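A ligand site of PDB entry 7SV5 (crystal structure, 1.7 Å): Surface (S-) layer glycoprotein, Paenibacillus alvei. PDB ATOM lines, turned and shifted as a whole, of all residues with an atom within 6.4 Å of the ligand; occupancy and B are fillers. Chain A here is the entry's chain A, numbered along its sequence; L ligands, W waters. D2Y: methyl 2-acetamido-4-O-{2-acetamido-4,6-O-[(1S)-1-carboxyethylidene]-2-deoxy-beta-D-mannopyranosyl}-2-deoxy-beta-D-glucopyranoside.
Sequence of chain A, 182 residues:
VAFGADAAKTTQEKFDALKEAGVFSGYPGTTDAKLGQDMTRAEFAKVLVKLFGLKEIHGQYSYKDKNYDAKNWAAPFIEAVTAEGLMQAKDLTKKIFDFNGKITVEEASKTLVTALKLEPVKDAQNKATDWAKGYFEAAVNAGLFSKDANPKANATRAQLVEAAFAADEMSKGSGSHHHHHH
N of Ser 25 sits at hydrogen-bond distance from OAS of the ligand, 2.7 Å away.
OG of Ser 25 sits at hydrogen-bond distance from O3 of the ligand, at 2.9 Å.
OAR of the ligand lies within salt-bridge range of NH2 of Arg 157, 2.8 Å away.
An oxygen (OAS) of the ligand lies within salt-bridge range of the side-chain amino group of Lys 46, 2.9 Å away.
OAR of the ligand lies within hydrogen-bond range of N of Gly 26, at 3.2 Å.
The backbone carbonyl oxygen of Gly 26 is in hydrogen-bond range of a nitrogen (N2) of the ligand.
The side-chain hydroxyl (OG) of Ser 25 is in hydrogen-bond range of the side-chain amino group (NZ) of Lys 46 (3.4 Å).
The guanidinium group (NH1) of Arg 157 lies within salt-bridge range of the side-chain carboxylate (OE1) of Glu 43 (3.2 Å).
The guanidinium group (NH1) of Arg 157 lies within hydrogen-bond range of the side-chain hydroxyl (OH) of Tyr 27, 3.3 Å away.
The guanidinium group (NE) of Arg 157 sits close to the backbone carbonyl oxygen (O) of Lys 34 (3.4 Å).
NE of Arg 157 lies within hydrogen-bond range of O of Ala 33, 2.9 Å away.
The side-chain carboxylate of Glu 43 lies within hydrogen-bond range of the side-chain hydroxyl of Tyr 27 (2.6 Å).
Water W3 lies within hydrogen-bond range of the side-chain carboxylate of Glu 43 (2.6 Å) and an oxygen (OBA) of the ligand (2.7 Å).
Residues that only touch the ligand: Phe 24, Tyr 27, Pro 28, Glu 43, Val 47 and Trp 73.
Hydrophobic or aromatic side chains that line the ligand: Phe 24, Tyr 27, Pro 28, Val 47 and Trp 73.
Of the 19 residues printed, 10 come within 4 Å of the ligand.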
ATOM      1  N   PHE A  15      19.561 -24.209 -17.328  1.00  0.00           N
ATOM      2  CA  PHE A  15      18.406 -25.028 -17.757  1.00  0.00           C
ATOM      3  C   PHE A  15      18.901 -26.423 -18.156  1.00  0.00           C
ATOM      4  O   PHE A  15      18.338 -27.430 -17.697  1.00  0.00           O
ATOM      5  CB  PHE A  15      17.639 -24.365 -18.897  1.00  0.00           C
ATOM      6  CG  PHE A  15      16.574 -25.244 -19.498  1.00  0.00           C
ATOM      7  CD1 PHE A  15      16.887 -26.130 -20.519  1.00  0.00           C
ATOM      8  CD2 PHE A  15      15.278 -25.221 -19.017  1.00  0.00           C
ATOM      9  CE1 PHE A  15      15.910 -26.958 -21.055  1.00  0.00           C
ATOM     10  CE2 PHE A  15      14.304 -26.044 -19.566  1.00  0.00           C
ATOM     11  CZ  PHE A  15      14.621 -26.908 -20.587  1.00  0.00           C
ATOM     12  N   VAL A  23      15.125 -31.759 -12.970  1.00  0.00           N
ATOM     13  CA  VAL A  23      14.292 -30.653 -12.389  1.00  0.00           C
ATOM     14  C   VAL A  23      13.449 -30.037 -13.505  1.00  0.00           C
ATOM     15  O   VAL A  23      12.259 -29.771 -13.270  1.00  0.00           O
ATOM     16  CB  VAL A  23      15.152 -29.603 -11.667  1.00  0.00           C
ATOM     17  CG1 VAL A  23      14.323 -28.404 -11.224  1.00  0.00           C
ATOM     18  CG2 VAL A  23      15.875 -30.206 -10.472  1.00  0.00           C
ATOM     19  N   PHE A  24      14.040 -29.795 -14.678  1.00  0.00           N
ATOM     20  CA  PHE A  24      13.338 -29.331 -15.890  1.00  0.00           C
ATOM     21  C   PHE A  24      13.338 -30.451 -16.936  1.00  0.00           C
ATOM     22  O   PHE A  24      14.167 -31.374 -16.842  1.00  0.00           O
ATOM     23  CB  PHE A  24      13.989 -28.068 -16.456  1.00  0.00           C
ATOM     24  CG  PHE A  24      13.608 -26.800 -15.728  1.00  0.00           C
ATOM     25  CD1 PHE A  24      14.166 -26.498 -14.496  1.00  0.00           C
ATOM     26  CD2 PHE A  24      12.670 -25.930 -16.262  1.00  0.00           C
ATOM     27  CE1 PHE A  24      13.799 -25.340 -13.823  1.00  0.00           C
ATOM     28  CE2 PHE A  24      12.312 -24.773 -15.588  1.00  0.00           C
ATOM     29  CZ  PHE A  24      12.882 -24.481 -14.371  1.00  0.00           C
ATOM     30  N   SER A  25      12.423 -30.371 -17.902  1.00  0.00           N
ATOM     31  CA  SER A  25      12.348 -31.285 -19.064  1.00  0.00           C
ATOM     32  C   SER A  25      12.014 -30.525 -20.353  1.00  0.00           C
ATOM     33  O   SER A  25      12.048 -31.165 -21.424  1.00  0.00           O
ATOM     34  CB  SER A  25      11.343 -32.387 -18.797  1.00  0.00           C
ATOM     35  OG  SER A  25      10.067 -31.854 -18.528  1.00  0.00           O
ATOM     36  N   GLY A  26      11.730 -29.230 -20.282  1.00  0.00           N
ATOM     37  CA  GLY A  26      11.256 -28.446 -21.433  1.00  0.00           C
ATOM     38  C   GLY A  26       9.901 -28.932 -21.922  1.00  0.00           C
ATOM     39  O   GLY A  26       9.128 -29.484 -21.101  1.00  0.00           O
ATOM     40  N   TYR A  27       9.616 -28.729 -23.204  1.00  0.00           N
ATOM     41  CA  TYR A  27       8.297 -29.009 -23.838  1.00  0.00           C
ATOM     42  C   TYR A  27       8.451 -30.173 -24.819  1.00  0.00           C
ATOM     43  O   TYR A  27       9.465 -30.281 -25.497  1.00  0.00           O
ATOM     44  CB  TYR A  27       7.786 -27.763 -24.562  1.00  0.00           C
ATOM     45  CG  TYR A  27       7.500 -26.602 -23.643  1.00  0.00           C
ATOM     46  CD1 TYR A  27       8.505 -25.697 -23.313  1.00  0.00           C
ATOM     47  CD2 TYR A  27       6.241 -26.414 -23.106  1.00  0.00           C
ATOM     48  CE1 TYR A  27       8.249 -24.634 -22.464  1.00  0.00           C
ATOM     49  CE2 TYR A  27       5.975 -25.350 -22.259  1.00  0.00           C
ATOM     50  CZ  TYR A  27       6.988 -24.459 -21.932  1.00  0.00           C
ATOM     51  OH  TYR A  27       6.719 -23.417 -21.085  1.00  0.00           O
ATOM     52  N   PRO A  28       7.434 -31.055 -24.937  1.00  0.00           N
ATOM     53  CA  PRO A  28       7.478 -32.134 -25.919  1.00  0.00           C
ATOM     54  C   PRO A  28       7.566 -31.576 -27.343  1.00  0.00           C
ATOM     55  O   PRO A  28       6.916 -30.591 -27.637  1.00  0.00           O
ATOM     56  CB  PRO A  28       6.163 -32.898 -25.719  1.00  0.00           C
ATOM     57  CG  PRO A  28       5.664 -32.471 -24.354  1.00  0.00           C
ATOM     58  CD  PRO A  28       6.189 -31.057 -24.143  1.00  0.00           C
ATOM     59  N   ALA A  33      13.476 -24.053 -24.813  1.00  0.00           N
ATOM     60  CA  ALA A  33      13.182 -23.961 -23.363  1.00  0.00           C
ATOM     61  C   ALA A  33      12.168 -22.845 -23.083  1.00  0.00           C
ATOM     62  O   ALA A  33      11.602 -22.840 -21.976  1.00  0.00           O
ATOM     63  CB  ALA A  33      14.458 -23.751 -22.586  1.00  0.00           C
ATOM     64  N   LYS A  34      11.944 -21.944 -24.057  1.00  0.00           N
ATOM     65  CA  LYS A  34      10.965 -20.816 -23.972  1.00  0.00           C
ATOM     66  C   LYS A  34      11.289 -19.977 -22.728  1.00  0.00           C
ATOM     67  O   LYS A  34      10.362 -19.631 -21.977  1.00  0.00           O
ATOM     68  CB  LYS A  34       9.522 -21.332 -23.948  1.00  0.00           C
ATOM     69  CG  LYS A  34       9.159 -22.239 -25.118  1.00  0.00           C
ATOM     70  CD  LYS A  34       7.668 -22.471 -25.268  1.00  0.00           C
ATOM     71  CE  LYS A  34       7.318 -23.632 -26.171  1.00  0.00           C
ATOM     72  NZ  LYS A  34       5.918 -24.084 -25.961  1.00  0.00           N
ATOM     73  N   MET A  39       6.247 -18.113 -16.704  1.00  0.00           N
ATOM     74  CA  MET A  39       5.989 -19.485 -16.211  1.00  0.00           C
ATOM     75  C   MET A  39       4.539 -19.581 -15.736  1.00  0.00           C
ATOM     76  O   MET A  39       4.020 -18.585 -15.205  1.00  0.00           O
ATOM     77  CB  MET A  39       6.927 -19.859 -15.059  1.00  0.00           C
ATOM     78  CG  MET A  39       6.830 -21.321 -14.713  1.00  0.00           C
ATOM     79  SD  MET A  39       8.097 -21.917 -13.573  1.00  0.00           S
ATOM     80  CE  MET A  39       9.426 -22.296 -14.716  1.00  0.00           C
ATOM     81  N   ALA A  42       1.148 -24.199 -13.055  1.00  0.00           N
ATOM     82  CA  ALA A  42       1.348 -25.653 -13.294  1.00  0.00           C
ATOM     83  C   ALA A  42       2.854 -25.948 -13.382  1.00  0.00           C
ATOM     84  O   ALA A  42       3.339 -26.876 -12.676  1.00  0.00           O
ATOM     85  CB  ALA A  42       0.637 -26.080 -14.540  1.00  0.00           C
ATOM     86  N   GLU A  43       3.578 -25.185 -14.193  1.00  0.00           N
ATOM     87  CA  GLU A  43       5.045 -25.361 -14.391  1.00  0.00           C
ATOM     88  C   GLU A  43       5.760 -25.155 -13.055  1.00  0.00           C
ATOM     89  O   GLU A  43       6.662 -25.951 -12.721  1.00  0.00           O
ATOM     90  CB  GLU A  43       5.540 -24.399 -15.469  1.00  0.00           C
ATOM     91  CG  GLU A  43       5.055 -24.786 -16.862  1.00  0.00           C
ATOM     92  CD  GLU A  43       5.354 -23.796 -17.970  1.00  0.00           C
ATOM     93  OE1 GLU A  43       5.799 -22.666 -17.659  1.00  0.00           O
ATOM     94  OE2 GLU A  43       5.116 -24.143 -19.135  1.00  0.00           O
ATOM     95  N   PHE A  44       5.369 -24.141 -12.290  1.00  0.00           N
ATOM     96  CA  PHE A  44       5.972 -23.834 -10.975  1.00  0.00           C
ATOM     97  C   PHE A  44       5.737 -25.000 -10.008  1.00  0.00           C
ATOM     98  O   PHE A  44       6.691 -25.392  -9.319  1.00  0.00           O
ATOM     99  CB  PHE A  44       5.430 -22.513 -10.420  1.00  0.00           C
ATOM    100  CG  PHE A  44       6.163 -21.971  -9.230  1.00  0.00           C
ATOM    101  CD1 PHE A  44       7.546 -21.913  -9.198  1.00  0.00           C
ATOM    102  CD2 PHE A  44       5.461 -21.485  -8.125  1.00  0.00           C
ATOM    103  CE1 PHE A  44       8.213 -21.385  -8.100  1.00  0.00           C
ATOM    104  CE2 PHE A  44       6.130 -20.962  -7.036  1.00  0.00           C
ATOM    105  CZ  PHE A  44       7.508 -20.903  -7.028  1.00  0.00           C
ATOM    106  N   LYS A  46       5.397 -28.152 -10.756  1.00  0.00           N
ATOM    107  CA  LYS A  46       6.304 -29.242 -11.187  1.00  0.00           C
ATOM    108  C   LYS A  46       7.714 -28.971 -10.639  1.00  0.00           C
ATOM    109  O   LYS A  46       8.289 -29.871  -9.991  1.00  0.00           O
ATOM    110  CB  LYS A  46       6.300 -29.410 -12.707  1.00  0.00           C
ATOM    111  CG  LYS A  46       6.842 -30.733 -13.216  1.00  0.00           C
ATOM    112  CD  LYS A  46       8.349 -30.853 -13.223  1.00  0.00           C
ATOM    113  CE  LYS A  46       9.027 -29.994 -14.269  1.00  0.00           C
ATOM    114  NZ  LYS A  46       9.582 -30.795 -15.380  1.00  0.00           N
ATOM    115  N   VAL A  47       8.241 -27.755 -10.869  1.00  0.00           N
ATOM    116  CA  VAL A  47       9.632 -27.391 -10.449  1.00  0.00           C
ATOM    117  C   VAL A  47       9.736 -27.543  -8.923  1.00  0.00           C
ATOM    118  O   VAL A  47      10.767 -28.069  -8.449  1.00  0.00           O
ATOM    119  CB  VAL A  47      10.017 -25.973 -10.914  1.00  0.00           C
ATOM    120  CG1 VAL A  47      11.367 -25.557 -10.357  1.00  0.00           C
ATOM    121  CG2 VAL A  47       9.999 -25.849 -12.426  1.00  0.00           C
ATOM    122  N   TRP A  73      -1.443 -33.107 -17.439  1.00  0.00           N
ATOM    123  CA  TRP A  73      -0.071 -33.537 -17.070  1.00  0.00           C
ATOM    124  C   TRP A  73       0.328 -32.995 -15.688  1.00  0.00           C
ATOM    125  O   TRP A  73       1.140 -33.644 -15.023  1.00  0.00           O
ATOM    126  CB  TRP A  73       0.934 -33.112 -18.145  1.00  0.00           C
ATOM    127  CG  TRP A  73       1.162 -31.630 -18.179  1.00  0.00           C
ATOM    128  CD1 TRP A  73       0.525 -30.720 -18.964  1.00  0.00           C
ATOM    129  CD2 TRP A  73       2.072 -30.889 -17.359  1.00  0.00           C
ATOM    130  NE1 TRP A  73       0.982 -29.456 -18.698  1.00  0.00           N
ATOM    131  CE2 TRP A  73       1.935 -29.525 -17.710  1.00  0.00           C
ATOM    132  CE3 TRP A  73       2.985 -31.233 -16.350  1.00  0.00           C
ATOM    133  CZ2 TRP A  73       2.678 -28.520 -17.104  1.00  0.00           C
ATOM    134  CZ3 TRP A  73       3.716 -30.235 -15.742  1.00  0.00           C
ATOM    135  CH2 TRP A  73       3.571 -28.896 -16.126  1.00  0.00           C
ATOM    136  N   PHE A  77       1.531 -32.969  -9.788  1.00  0.00           N
ATOM    137  CA  PHE A  77       2.411 -31.942  -9.175  1.00  0.00           C
ATOM    138  C   PHE A  77       1.563 -30.925  -8.405  1.00  0.00           C
ATOM    139  O   PHE A  77       1.981 -30.524  -7.310  1.00  0.00           O
ATOM    140  CB  PHE A  77       3.254 -31.259 -10.256  1.00  0.00           C
ATOM    141  CG  PHE A  77       4.057 -32.240 -11.073  1.00  0.00           C
ATOM    142  CD1 PHE A  77       5.200 -32.827 -10.542  1.00  0.00           C
ATOM    143  CD2 PHE A  77       3.650 -32.612 -12.340  1.00  0.00           C
ATOM    144  CE1 PHE A  77       5.919 -33.755 -11.273  1.00  0.00           C
ATOM    145  CE2 PHE A  77       4.361 -33.539 -13.072  1.00  0.00           C
ATOM    146  CZ  PHE A  77       5.498 -34.102 -12.543  1.00  0.00           C
ATOM    147  N   ASN A 100      -3.131 -22.467 -15.663  1.00  0.00           N
ATOM    148  CA  ASN A 100      -2.542 -21.674 -16.778  1.00  0.00           C
ATOM    149  C   ASN A 100      -2.115 -20.297 -16.290  1.00  0.00           C
ATOM    150  O   ASN A 100      -1.413 -19.594 -17.050  1.00  0.00           O
ATOM    151  CB  ASN A 100      -3.490 -21.532 -17.971  1.00  0.00           C
ATOM    152  CG  ASN A 100      -3.659 -22.812 -18.755  1.00  0.00           C
ATOM    153  OD1 ASN A 100      -2.713 -23.590 -18.888  1.00  0.00           O
ATOM    154  ND2 ASN A 100      -4.847 -23.030 -19.279  1.00  0.00           N
ATOM    155  N   ARG A 157      10.293 -17.824 -17.267  1.00  0.00           N
ATOM    156  CA  ARG A 157      10.928 -19.164 -17.179  1.00  0.00           C
ATOM    157  C   ARG A 157      12.430 -18.978 -16.925  1.00  0.00           C
ATOM    158  O   ARG A 157      12.972 -19.732 -16.107  1.00  0.00           O
ATOM    159  CB  ARG A 157      10.590 -19.969 -18.430  1.00  0.00           C
ATOM    160  CG  ARG A 157       9.135 -20.432 -18.447  1.00  0.00           C
ATOM    161  CD  ARG A 157       8.757 -21.172 -19.704  1.00  0.00           C
ATOM    162  NE  ARG A 157       9.655 -22.283 -19.968  1.00  0.00           N
ATOM    163  CZ  ARG A 157       9.598 -23.472 -19.359  1.00  0.00           C
ATOM    164  NH1 ARG A 157       8.687 -23.719 -18.430  1.00  0.00           N
ATOM    165  NH2 ARG A 157      10.487 -24.403 -19.682  1.00  0.00           N
HETATM  166  C4  D2Y L   1       7.311 -29.171 -18.183  1.00  0.00           C
HETATM  167  C5  D2Y L   1       6.406 -28.188 -18.872  1.00  0.00           C
HETATM  168  C6  D2Y L   1       7.211 -26.920 -19.194  1.00  0.00           C
HETATM  169  C7  D2Y L   1       7.215 -32.570 -20.739  1.00  0.00           C
HETATM  170  C8  D2Y L   1       8.374 -32.771 -21.724  1.00  0.00           C
HETATM  171  N2  D2Y L   1       7.115 -31.353 -20.196  1.00  0.00           N
HETATM  172  C3  D2Y L   1       6.596 -30.466 -17.915  1.00  0.00           C
HETATM  173  O7  D2Y L   1       6.457 -33.496 -20.461  1.00  0.00           O
HETATM  174  C2  D2Y L   1       6.040 -31.030 -19.217  1.00  0.00           C
HETATM  175  O3  D2Y L   1       7.484 -31.376 -17.276  1.00  0.00           O
HETATM  176  O4  D2Y L   1       7.688 -28.589 -16.948  1.00  0.00           O
HETATM  177  CAO D2Y L   1       8.445 -27.371 -17.138  1.00  0.00           C
HETATM  178  CAQ D2Y L   1       8.684 -26.744 -15.764  1.00  0.00           C
HETATM  179  CAP D2Y L   1       9.819 -27.699 -17.735  1.00  0.00           C
HETATM  180  OAS D2Y L   1      10.419 -28.689 -17.264  1.00  0.00           O
HETATM  181  OAR D2Y L   1      10.226 -26.976 -18.647  1.00  0.00           O
HETATM  182  O6  D2Y L   1       7.722 -26.433 -17.983  1.00  0.00           O
HETATM  183  O5  D2Y L   1       5.899 -28.767 -20.081  1.00  0.00           O
HETATM  184  C1  D2Y L   1       5.146 -29.965 -19.799  1.00  0.00           C
HETATM  185  O1  D2Y L   1       4.668 -30.385 -21.063  1.00  0.00           O
HETATM  186  CAZ D2Y L   1       3.317 -30.020 -21.339  1.00  0.00           C
HETATM  187  CAY D2Y L   1       3.242 -28.692 -22.047  1.00  0.00           C
HETATM  188  OBA D2Y L   1       3.672 -27.643 -21.166  1.00  0.00           O
HETATM  189  CAU D2Y L   1       2.729 -31.101 -22.236  1.00  0.00           C
HETATM  190  CBB D2Y L   1       2.815 -32.452 -21.549  1.00  0.00           C
HETATM  191  OBC D2Y L   1       2.217 -33.420 -22.403  1.00  0.00           O
HETATM  192  OAV D2Y L   1       1.353 -30.801 -22.495  1.00  0.00           O
HETATM  193  CAW D2Y L   1       1.226 -29.577 -23.235  1.00  0.00           C
HETATM  194  OBD D2Y L   1      -0.161 -29.326 -23.436  1.00  0.00           O
HETATM  195  CBI D2Y L   1      -0.794 -30.358 -24.229  1.00  0.00           C
HETATM  196  CAX D2Y L   1       1.808 -28.415 -22.437  1.00  0.00           C
HETATM  197  NBE D2Y L   1       1.753 -27.219 -23.290  1.00  0.00           N
HETATM  198  CBF D2Y L   1       0.960 -26.170 -23.025  1.00  0.00           C
HETATM  199  OBH D2Y L   1       0.214 -26.055 -22.054  1.00  0.00           O
HETATM  200  CBG D2Y L   1       1.057 -25.044 -24.059  1.00  0.00           C
HETATM  201  O   HOH W   1      -0.371 -33.673 -21.786  1.00  0.00           O
HETATM  202  O   HOH W   2       3.720 -27.410 -25.572  1.00  0.00           O
HETATM  203  O   HOH W   3       2.893 -25.421 -19.780  1.00  0.00           O
HETATM  204  O   HOH W   4       6.071 -33.513 -16.471  1.00  0.00           O
HETATM  205  O   HOH W   5       6.274 -35.852 -21.773  1.00  0.00           O
